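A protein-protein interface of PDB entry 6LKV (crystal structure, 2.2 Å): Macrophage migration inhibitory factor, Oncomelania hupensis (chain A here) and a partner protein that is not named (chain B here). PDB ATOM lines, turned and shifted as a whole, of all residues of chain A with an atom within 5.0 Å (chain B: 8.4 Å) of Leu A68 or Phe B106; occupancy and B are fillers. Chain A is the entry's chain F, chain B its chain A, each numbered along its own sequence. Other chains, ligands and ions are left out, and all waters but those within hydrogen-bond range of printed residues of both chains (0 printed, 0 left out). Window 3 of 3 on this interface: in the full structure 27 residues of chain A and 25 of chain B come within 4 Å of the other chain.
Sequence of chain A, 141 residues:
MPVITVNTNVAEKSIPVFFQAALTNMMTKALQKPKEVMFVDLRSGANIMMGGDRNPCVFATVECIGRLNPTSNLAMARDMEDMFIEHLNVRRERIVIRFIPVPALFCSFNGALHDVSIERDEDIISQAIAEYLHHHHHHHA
Of chain B, only Phe B106 (3.7 Å) comes within 4 Å of Leu A68.
Printed residues of chain A within 4 Å of Phe B106: Leu A68, Asn A73, Arg A98, Phe A99 and Pro A101.
Printed residues of chain A within 4 Å of Cys B107: Ile A97 (3.2 Å).
Printed residues of chain A within 4 Å of Val B102: Arg A98 (3.9 Å).
Val A62 touches none of the printed residues of chain B.
The nearest residue of chain B that does not touch Leu A68 is Leu B105 (6.9 Å).
The nearest residue of chain A that does not touch Phe B106 is Asn A69 (4.04 Å).
The nearest printed residue of chain A that does not touch Leu B113 is Asn A73 (4.3 Å).
Among the printed residues, merely in contact across the chains: Leu A68 with Phe B106 (3.7 Å), Pro A70 with Leu B105 (3.7 Å), Pro A70 with Leu B113 (3.3 Å), Asn A73 with Phe B106 (3.5 Å), Arg A98 with Val B102 (3.9 Å), Arg A98 with Phe B106 (3.5 Å) and Pro A101 with Phe B106 (3.6 Å).
N of Val A62 lies within hydrogen-bond range of O of Arg A98, at 2.9 Å.
The side-chain amide nitrogen (ND2) of Asn A73 lies close to the backbone carbonyl oxygen (O) of Asn A69, at 3.2 Å.
The backbone carbonyl oxygen (O) of Cys B107 is in hydrogen-bond range of a ring nitrogen (ND1) of His B114 (2.7 Å).
Along chain B the printed residues that touch a printed residue of chain A span positions 102 to 113.
Among the printed residues, 11 pairs touch across the chains.
Among the printed residues, no Asp or Glu carboxylate lies within 4 Å of a Lys or Arg side-chain nitrogen of the other chain.
The side-chain amide nitrogen (ND2) of Asn A73 sits at hydrogen-bond distance from the backbone carbonyl oxygen (O) of Leu B105.
O of Ile A97 lies close to SG of Cys B107, at 3.6 Å.
The backbone carbonyl oxygen (O) of Ile A97 is in hydrogen-bond range of the backbone NH (N) of Ser B108 (2.8 Å).
N of Phe A99 lies within hydrogen-bond range of O of Phe B106, at 2.8 Å.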
ATOM      1  N   LEU A  31     -16.077 -19.462   7.188  1.00  0.00           N
ATOM      2  CA  LEU A  31     -16.515 -20.617   7.998  1.00  0.00           C
ATOM      3  C   LEU A  31     -15.818 -21.899   7.512  1.00  0.00           C
ATOM      4  O   LEU A  31     -16.013 -22.957   8.167  1.00  0.00           O
ATOM      5  CB  LEU A  31     -18.038 -20.763   7.912  1.00  0.00           C
ATOM      6  CG  LEU A  31     -18.870 -19.674   8.593  1.00  0.00           C
ATOM      7  CD1 LEU A  31     -20.349 -19.929   8.328  1.00  0.00           C
ATOM      8  CD2 LEU A  31     -18.608 -19.628  10.100  1.00  0.00           C
ATOM      9  N   VAL A  62     -26.193 -16.619  12.112  1.00  0.00           N
ATOM     10  CA  VAL A  62     -25.247 -17.575  11.488  1.00  0.00           C
ATOM     11  C   VAL A  62     -25.399 -18.898  12.229  1.00  0.00           C
ATOM     12  O   VAL A  62     -24.978 -18.958  13.406  1.00  0.00           O
ATOM     13  CB  VAL A  62     -23.806 -17.034  11.550  1.00  0.00           C
ATOM     14  CG1 VAL A  62     -22.847 -18.035  10.901  1.00  0.00           C
ATOM     15  CG2 VAL A  62     -23.689 -15.670  10.891  1.00  0.00           C
ATOM     16  N   CYS A  64     -24.226 -22.750  12.260  1.00  0.00           N
ATOM     17  CA  CYS A  64     -23.020 -23.447  11.770  1.00  0.00           C
ATOM     18  C   CYS A  64     -22.626 -24.561  12.737  1.00  0.00           C
ATOM     19  O   CYS A  64     -22.672 -24.334  13.976  1.00  0.00           O
ATOM     20  CB  CYS A  64     -21.872 -22.456  11.611  1.00  0.00           C
ATOM     21  SG  CYS A  64     -20.480 -23.165  10.690  1.00  0.00           S
ATOM     22  N   GLY A  66     -19.624 -26.381  14.311  1.00  0.00           N
ATOM     23  CA  GLY A  66     -18.260 -25.920  14.584  1.00  0.00           C
ATOM     24  C   GLY A  66     -18.058 -24.473  14.190  1.00  0.00           C
ATOM     25  O   GLY A  66     -19.071 -23.736  13.984  1.00  0.00           O
ATOM     26  N   ARG A  67     -16.790 -24.057  14.155  1.00  0.00           N
ATOM     27  CA  ARG A  67     -16.275 -22.803  13.549  1.00  0.00           C
ATOM     28  C   ARG A  67     -16.560 -21.587  14.433  1.00  0.00           C
ATOM     29  O   ARG A  67     -15.779 -20.628  14.358  1.00  0.00           O
ATOM     30  CB  ARG A  67     -16.872 -22.568  12.161  1.00  0.00           C
ATOM     31  CG  ARG A  67     -16.764 -23.766  11.230  1.00  0.00           C
ATOM     32  CD  ARG A  67     -15.308 -24.126  10.984  1.00  0.00           C
ATOM     33  NE  ARG A  67     -15.146 -25.035   9.857  1.00  0.00           N
ATOM     34  CZ  ARG A  67     -15.035 -26.362   9.937  1.00  0.00           C
ATOM     35  NH1 ARG A  67     -15.073 -26.989  11.107  1.00  0.00           N
ATOM     36  NH2 ARG A  67     -14.892 -27.059   8.824  1.00  0.00           N
ATOM     37  N   LEU A  68     -17.621 -21.598  15.238  1.00  0.00           N
ATOM     38  CA  LEU A  68     -18.037 -20.412  16.032  1.00  0.00           C
ATOM     39  C   LEU A  68     -17.348 -20.423  17.403  1.00  0.00           C
ATOM     40  O   LEU A  68     -17.494 -21.402  18.146  1.00  0.00           O
ATOM     41  CB  LEU A  68     -19.561 -20.405  16.175  1.00  0.00           C
ATOM     42  CG  LEU A  68     -20.352 -20.560  14.875  1.00  0.00           C
ATOM     43  CD1 LEU A  68     -21.859 -20.509  15.161  1.00  0.00           C
ATOM     44  CD2 LEU A  68     -19.947 -19.520  13.860  1.00  0.00           C
ATOM     45  N   ASN A  69     -16.661 -19.325  17.713  1.00  0.00           N
ATOM     46  CA  ASN A  69     -15.953 -19.079  18.994  1.00  0.00           C
ATOM     47  C   ASN A  69     -15.805 -17.573  19.125  1.00  0.00           C
ATOM     48  O   ASN A  69     -15.969 -16.847  18.152  1.00  0.00           O
ATOM     49  CB  ASN A  69     -14.605 -19.844  19.044  1.00  0.00           C
ATOM     50  CG  ASN A  69     -13.660 -19.389  17.966  1.00  0.00           C
ATOM     51  OD1 ASN A  69     -13.202 -18.250  17.989  1.00  0.00           O
ATOM     52  ND2 ASN A  69     -13.437 -20.236  16.971  1.00  0.00           N
ATOM     53  N   PRO A  70     -15.483 -17.049  20.323  1.00  0.00           N
ATOM     54  CA  PRO A  70     -15.419 -15.605  20.521  1.00  0.00           C
ATOM     55  C   PRO A  70     -14.559 -14.894  19.477  1.00  0.00           C
ATOM     56  O   PRO A  70     -14.942 -13.806  19.034  1.00  0.00           O
ATOM     57  CB  PRO A  70     -14.847 -15.477  21.947  1.00  0.00           C
ATOM     58  CG  PRO A  70     -15.363 -16.720  22.634  1.00  0.00           C
ATOM     59  CD  PRO A  70     -15.265 -17.798  21.571  1.00  0.00           C
ATOM     60  N   SER A  72     -13.473 -15.987  16.191  1.00  0.00           N
ATOM     61  CA  SER A  72     -14.047 -16.068  14.821  1.00  0.00           C
ATOM     62  C   SER A  72     -15.348 -15.228  14.753  1.00  0.00           C
ATOM     63  O   SER A  72     -15.542 -14.512  13.773  1.00  0.00           O
ATOM     64  CB  SER A  72     -14.227 -17.497  14.399  1.00  0.00           C
ATOM     65  OG  SER A  72     -15.225 -18.141  15.189  1.00  0.00           O
ATOM     66  N   ASN A  73     -16.155 -15.222  15.813  1.00  0.00           N
ATOM     67  CA  ASN A  73     -17.472 -14.515  15.838  1.00  0.00           C
ATOM     68  C   ASN A  73     -17.251 -13.011  15.636  1.00  0.00           C
ATOM     69  O   ASN A  73     -17.936 -12.432  14.775  1.00  0.00           O
ATOM     70  CB  ASN A  73     -18.232 -14.768  17.138  1.00  0.00           C
ATOM     71  CG  ASN A  73     -18.711 -16.187  17.278  1.00  0.00           C
ATOM     72  OD1 ASN A  73     -18.664 -16.955  16.320  1.00  0.00           O
ATOM     73  ND2 ASN A  73     -19.154 -16.540  18.470  1.00  0.00           N
ATOM     74  N   MET A  76     -15.977 -12.285  11.998  1.00  0.00           N
ATOM     75  CA  MET A  76     -17.056 -12.514  11.008  1.00  0.00           C
ATOM     76  C   MET A  76     -18.096 -11.404  11.151  1.00  0.00           C
ATOM     77  O   MET A  76     -18.525 -10.893  10.099  1.00  0.00           O
ATOM     78  CB  MET A  76     -17.702 -13.890  11.177  1.00  0.00           C
ATOM     79  CG  MET A  76     -16.825 -14.992  10.623  1.00  0.00           C
ATOM     80  SD  MET A  76     -17.567 -16.632  10.701  1.00  0.00           S
ATOM     81  CE  MET A  76     -17.701 -16.889  12.466  1.00  0.00           C
ATOM     82  N   ILE A  97     -25.997  -9.379  15.108  1.00  0.00           N
ATOM     83  CA  ILE A  97     -25.775 -10.726  14.525  1.00  0.00           C
ATOM     84  C   ILE A  97     -25.678 -11.710  15.684  1.00  0.00           C
ATOM     85  O   ILE A  97     -24.931 -11.447  16.655  1.00  0.00           O
ATOM     86  CB  ILE A  97     -24.519 -10.765  13.647  1.00  0.00           C
ATOM     87  CG1 ILE A  97     -24.525  -9.641  12.608  1.00  0.00           C
ATOM     88  CG2 ILE A  97     -24.369 -12.145  13.023  1.00  0.00           C
ATOM     89  CD1 ILE A  97     -23.159  -9.454  11.935  1.00  0.00           C
ATOM     90  N   ARG A  98     -26.434 -12.794  15.588  1.00  0.00           N
ATOM     91  CA  ARG A  98     -26.372 -13.906  16.544  1.00  0.00           C
ATOM     92  C   ARG A  98     -25.705 -15.085  15.840  1.00  0.00           C
ATOM     93  O   ARG A  98     -26.132 -15.455  14.727  1.00  0.00           O
ATOM     94  CB  ARG A  98     -27.769 -14.219  17.082  1.00  0.00           C
ATOM     95  CG  ARG A  98     -27.801 -15.398  18.029  1.00  0.00           C
ATOM     96  CD  ARG A  98     -29.216 -15.822  18.404  1.00  0.00           C
ATOM     97  NE  ARG A  98     -29.074 -17.118  19.012  1.00  0.00           N
ATOM     98  CZ  ARG A  98     -29.977 -18.090  19.010  1.00  0.00           C
ATOM     99  NH1 ARG A  98     -31.167 -17.933  18.455  1.00  0.00           N
ATOM    100  NH2 ARG A  98     -29.659 -19.254  19.544  1.00  0.00           N
ATOM    101  N   PHE A  99     -24.720 -15.671  16.516  1.00  0.00           N
ATOM    102  CA  PHE A  99     -23.940 -16.855  16.086  1.00  0.00           C
ATOM    103  C   PHE A  99     -24.519 -18.034  16.858  1.00  0.00           C
ATOM    104  O   PHE A  99     -24.593 -17.966  18.124  1.00  0.00           O
ATOM    105  CB  PHE A  99     -22.448 -16.588  16.330  1.00  0.00           C
ATOM    106  CG  PHE A  99     -21.909 -15.453  15.495  1.00  0.00           C
ATOM    107  CD1 PHE A  99     -21.472 -15.658  14.196  1.00  0.00           C
ATOM    108  CD2 PHE A  99     -21.883 -14.164  15.979  1.00  0.00           C
ATOM    109  CE1 PHE A  99     -21.008 -14.610  13.415  1.00  0.00           C
ATOM    110  CE2 PHE A  99     -21.422 -13.118  15.199  1.00  0.00           C
ATOM    111  CZ  PHE A  99     -20.979 -13.337  13.921  1.00  0.00           C
ATOM    112  N   ILE A 100     -24.975 -19.046  16.131  1.00  0.00           N
ATOM    113  CA  ILE A 100     -25.772 -20.174  16.671  1.00  0.00           C
ATOM    114  C   ILE A 100     -25.015 -21.464  16.403  1.00  0.00           C
ATOM    115  O   ILE A 100     -25.009 -21.984  15.275  1.00  0.00           O
ATOM    116  CB  ILE A 100     -27.190 -20.234  16.068  1.00  0.00           C
ATOM    117  CG1 ILE A 100     -27.906 -18.886  16.199  1.00  0.00           C
ATOM    118  CG2 ILE A 100     -27.976 -21.368  16.702  1.00  0.00           C
ATOM    119  CD1 ILE A 100     -29.363 -18.930  15.735  1.00  0.00           C
ATOM    120  N   PRO A 101     -24.380 -22.035  17.455  1.00  0.00           N
ATOM    121  CA  PRO A 101     -23.715 -23.328  17.336  1.00  0.00           C
ATOM    122  C   PRO A 101     -24.758 -24.418  17.114  1.00  0.00           C
ATOM    123  O   PRO A 101     -25.728 -24.445  17.828  1.00  0.00           O
ATOM    124  CB  PRO A 101     -23.042 -23.544  18.706  1.00  0.00           C
ATOM    125  CG  PRO A 101     -23.019 -22.186  19.341  1.00  0.00           C
ATOM    126  CD  PRO A 101     -24.241 -21.453  18.797  1.00  0.00           C
ATOM    127  N   MET B   1     -29.936  -9.872  19.734  1.00  0.00           N
ATOM    128  CA  MET B   1     -30.698  -9.726  20.962  1.00  0.00           C
ATOM    129  C   MET B   1     -30.769  -8.252  21.410  1.00  0.00           C
ATOM    130  O   MET B   1     -29.903  -7.439  21.035  1.00  0.00           O
ATOM    131  CB  MET B   1     -30.036 -10.615  22.020  1.00  0.00           C
ATOM    132  CG  MET B   1     -29.072  -9.845  22.892  1.00  0.00           C
ATOM    133  SD  MET B   1     -29.859  -8.938  24.244  1.00  0.00           S
ATOM    134  CE  MET B   1     -28.636  -7.631  24.450  1.00  0.00           C
ATOM    135  N   ILE B  65     -29.581 -11.789  25.800  1.00  0.00           N
ATOM    136  CA  ILE B  65     -28.367 -12.103  26.616  1.00  0.00           C
ATOM    137  C   ILE B  65     -28.735 -11.812  28.071  1.00  0.00           C
ATOM    138  O   ILE B  65     -29.144 -10.685  28.360  1.00  0.00           O
ATOM    139  CB  ILE B  65     -27.159 -11.267  26.148  1.00  0.00           C
ATOM    140  CG1 ILE B  65     -26.893 -11.460  24.656  1.00  0.00           C
ATOM    141  CG2 ILE B  65     -25.926 -11.624  26.968  1.00  0.00           C
ATOM    142  CD1 ILE B  65     -26.003 -10.380  24.078  1.00  0.00           C
ATOM    143  N   PRO B 101     -31.912 -18.092  25.343  1.00  0.00           N
ATOM    144  CA  PRO B 101     -30.727 -17.502  25.938  1.00  0.00           C
ATOM    145  C   PRO B 101     -29.638 -17.365  24.880  1.00  0.00           C
ATOM    146  O   PRO B 101     -29.384 -18.297  24.192  1.00  0.00           O
ATOM    147  CB  PRO B 101     -30.268 -18.500  27.011  1.00  0.00           C
ATOM    148  CG  PRO B 101     -31.462 -19.378  27.238  1.00  0.00           C
ATOM    149  CD  PRO B 101     -32.189 -19.430  25.895  1.00  0.00           C
ATOM    150  N   VAL B 102     -29.044 -16.185  24.780  1.00  0.00           N
ATOM    151  CA  VAL B 102     -27.956 -15.897  23.803  1.00  0.00           C
ATOM    152  C   VAL B 102     -26.662 -15.691  24.590  1.00  0.00           C
ATOM    153  O   VAL B 102     -26.649 -14.905  25.537  1.00  0.00           O
ATOM    154  CB  VAL B 102     -28.333 -14.686  22.935  1.00  0.00           C
ATOM    155  CG1 VAL B 102     -27.236 -14.330  21.970  1.00  0.00           C
ATOM    156  CG2 VAL B 102     -29.665 -14.894  22.195  1.00  0.00           C
ATOM    157  N   PRO B 103     -25.561 -16.411  24.269  1.00  0.00           N
ATOM    158  CA  PRO B 103     -24.254 -16.142  24.890  1.00  0.00           C
ATOM    159  C   PRO B 103     -23.711 -14.782  24.458  1.00  0.00           C
ATOM    160  O   PRO B 103     -23.807 -14.452  23.260  1.00  0.00           O
ATOM    161  CB  PRO B 103     -23.306 -17.252  24.404  1.00  0.00           C
ATOM    162  CG  PRO B 103     -24.252 -18.308  23.820  1.00  0.00           C
ATOM    163  CD  PRO B 103     -25.490 -17.546  23.344  1.00  0.00           C
ATOM    164  N   ALA B 104     -23.136 -14.040  25.410  1.00  0.00           N
ATOM    165  CA  ALA B 104     -22.572 -12.682  25.208  1.00  0.00           C
ATOM    166  C   ALA B 104     -21.531 -12.682  24.085  1.00  0.00           C
ATOM    167  O   ALA B 104     -21.494 -11.703  23.307  1.00  0.00           O
ATOM    168  CB  ALA B 104     -21.996 -12.150  26.514  1.00  0.00           C
ATOM    169  N   LEU B 105     -20.728 -13.740  23.965  1.00  0.00           N
ATOM    170  CA  LEU B 105     -19.631 -13.786  22.962  1.00  0.00           C
ATOM    171  C   LEU B 105     -20.117 -14.460  21.674  1.00  0.00           C
ATOM    172  O   LEU B 105     -19.280 -14.673  20.771  1.00  0.00           O
ATOM    173  CB  LEU B 105     -18.426 -14.531  23.566  1.00  0.00           C
ATOM    174  CG  LEU B 105     -17.867 -13.932  24.867  1.00  0.00           C
ATOM    175  CD1 LEU B 105     -16.718 -14.789  25.431  1.00  0.00           C
ATOM    176  CD2 LEU B 105     -17.419 -12.501  24.640  1.00  0.00           C
ATOM    177  N   PHE B 106     -21.430 -14.729  21.558  1.00  0.00           N
ATOM    178  CA  PHE B 106     -22.052 -15.320  20.345  1.00  0.00           C
ATOM    179  C   PHE B 106     -23.069 -14.331  19.754  1.00  0.00           C
ATOM    180  O   PHE B 106     -23.981 -14.720  19.008  1.00  0.00           O
ATOM    181  CB  PHE B 106     -22.606 -16.703  20.684  1.00  0.00           C
ATOM    182  CG  PHE B 106     -21.549 -17.779  20.741  1.00  0.00           C
ATOM    183  CD1 PHE B 106     -20.578 -17.789  21.743  1.00  0.00           C
ATOM    184  CD2 PHE B 106     -21.491 -18.769  19.780  1.00  0.00           C
ATOM    185  CE1 PHE B 106     -19.552 -18.726  21.734  1.00  0.00           C
ATOM    186  CE2 PHE B 106     -20.481 -19.728  19.794  1.00  0.00           C
ATOM    187  CZ  PHE B 106     -19.523 -19.722  20.782  1.00  0.00           C
ATOM    188  N   CYS B 107     -22.883 -13.051  20.046  1.00  0.00           N
ATOM    189  CA  CYS B 107     -23.786 -11.971  19.611  1.00  0.00           C
ATOM    190  C   CYS B 107     -23.012 -10.657  19.478  1.00  0.00           C
ATOM    191  O   CYS B 107     -22.459 -10.176  20.514  1.00  0.00           O
ATOM    192  CB  CYS B 107     -24.954 -11.832  20.573  1.00  0.00           C
ATOM    193  SG  CYS B 107     -26.207 -10.683  19.945  1.00  0.00           S
ATOM    194  N   SER B 108     -23.006 -10.095  18.263  1.00  0.00           N
ATOM    195  CA  SER B 108     -22.401  -8.773  17.938  1.00  0.00           C
ATOM    196  C   SER B 108     -23.447  -7.648  17.948  1.00  0.00           C
ATOM    197  O   SER B 108     -24.615  -7.888  17.570  1.00  0.00           O
ATOM    198  CB  SER B 108     -21.667  -8.813  16.639  1.00  0.00           C
ATOM    199  OG  SER B 108     -22.523  -9.097  15.550  1.00  0.00           O
ATOM    200  N   PHE B 109     -23.040  -6.474  18.425  1.00  0.00           N
ATOM    201  CA  PHE B 109     -23.711  -5.182  18.199  1.00  0.00           C
ATOM    202  C   PHE B 109     -22.635  -4.131  17.926  1.00  0.00           C
ATOM    203  O   PHE B 109     -21.679  -4.035  18.728  1.00  0.00           O
ATOM    204  CB  PHE B 109     -24.554  -4.797  19.414  1.00  0.00           C
ATOM    205  CG  PHE B 109     -25.012  -3.368  19.380  1.00  0.00           C
ATOM    206  CD1 PHE B 109     -25.750  -2.893  18.299  1.00  0.00           C
ATOM    207  CD2 PHE B 109     -24.666  -2.487  20.390  1.00  0.00           C
ATOM    208  CE1 PHE B 109     -26.175  -1.573  18.258  1.00  0.00           C
ATOM    209  CE2 PHE B 109     -25.083  -1.156  20.346  1.00  0.00           C
ATOM    210  CZ  PHE B 109     -25.839  -0.707  19.284  1.00  0.00           C
ATOM    211  N   ALA B 112     -18.677  -4.977  17.943  1.00  0.00           N
ATOM    212  CA  ALA B 112     -18.116  -5.682  19.122  1.00  0.00           C
ATOM    213  C   ALA B 112     -19.072  -6.776  19.606  1.00  0.00           C
ATOM    214  O   ALA B 112     -20.289  -6.709  19.302  1.00  0.00           O
ATOM    215  CB  ALA B 112     -17.845  -4.694  20.243  1.00  0.00           C
ATOM    216  N   LEU B 113     -18.559  -7.736  20.373  1.00  0.00           N
ATOM    217  CA  LEU B 113     -19.387  -8.727  21.090  1.00  0.00           C
ATOM    218  C   LEU B 113     -19.921  -8.066  22.355  1.00  0.00           C
ATOM    219  O   LEU B 113     -19.850  -6.826  22.444  1.00  0.00           O
ATOM    220  CB  LEU B 113     -18.591  -9.990  21.394  1.00  0.00           C
ATOM    221  CG  LEU B 113     -17.872 -10.623  20.204  1.00  0.00           C
ATOM    222  CD1 LEU B 113     -17.108 -11.850  20.653  1.00  0.00           C
ATOM    223  CD2 LEU B 113     -18.831 -10.956  19.076  1.00  0.00           C
ATOM    224  N   HIS B 114     -20.505  -8.849  23.261  1.00  0.00           N
ATOM    225  CA  HIS B 114     -21.087  -8.330  24.514  1.00  0.00           C
ATOM    226  C   HIS B 114     -20.246  -8.827  25.689  1.00  0.00           C
ATOM    227  O   HIS B 114     -19.558  -9.844  25.561  1.00  0.00           O
ATOM    228  CB  HIS B 114     -22.563  -8.747  24.628  1.00  0.00           C
ATOM    229  CG  HIS B 114     -23.455  -8.092  23.630  1.00  0.00           C
ATOM    230  ND1 HIS B 114     -23.518  -8.515  22.307  1.00  0.00           N
ATOM    231  CD2 HIS B 114     -24.340  -7.082  23.760  1.00  0.00           C
ATOM    232  CE1 HIS B 114     -24.393  -7.763  21.660  1.00  0.00           C
ATOM    233  NE2 HIS B 114     -24.919  -6.882  22.543  1.00  0.00           N
ATOM    234  N   GLU B 119     -24.703 -12.057  30.974  1.00  0.00           N
ATOM    235  CA  GLU B 119     -25.372 -13.386  30.964  1.00  0.00           C
ATOM    236  C   GLU B 119     -25.920 -13.707  32.345  1.00  0.00           C
ATOM    237  O   GLU B 119     -26.982 -14.403  32.407  1.00  0.00           O
ATOM    238  CB  GLU B 119     -24.464 -14.532  30.562  1.00  0.00           C
ATOM    239  CG  GLU B 119     -24.071 -14.530  29.097  1.00  0.00           C
ATOM    240  CD  GLU B 119     -23.051 -15.609  28.776  1.00  0.00           C
ATOM    241  OE1 GLU B 119     -22.729 -16.373  29.690  1.00  0.00           O
ATOM    242  OE2 GLU B 119     -22.522 -15.622  27.665  1.00  0.00           O
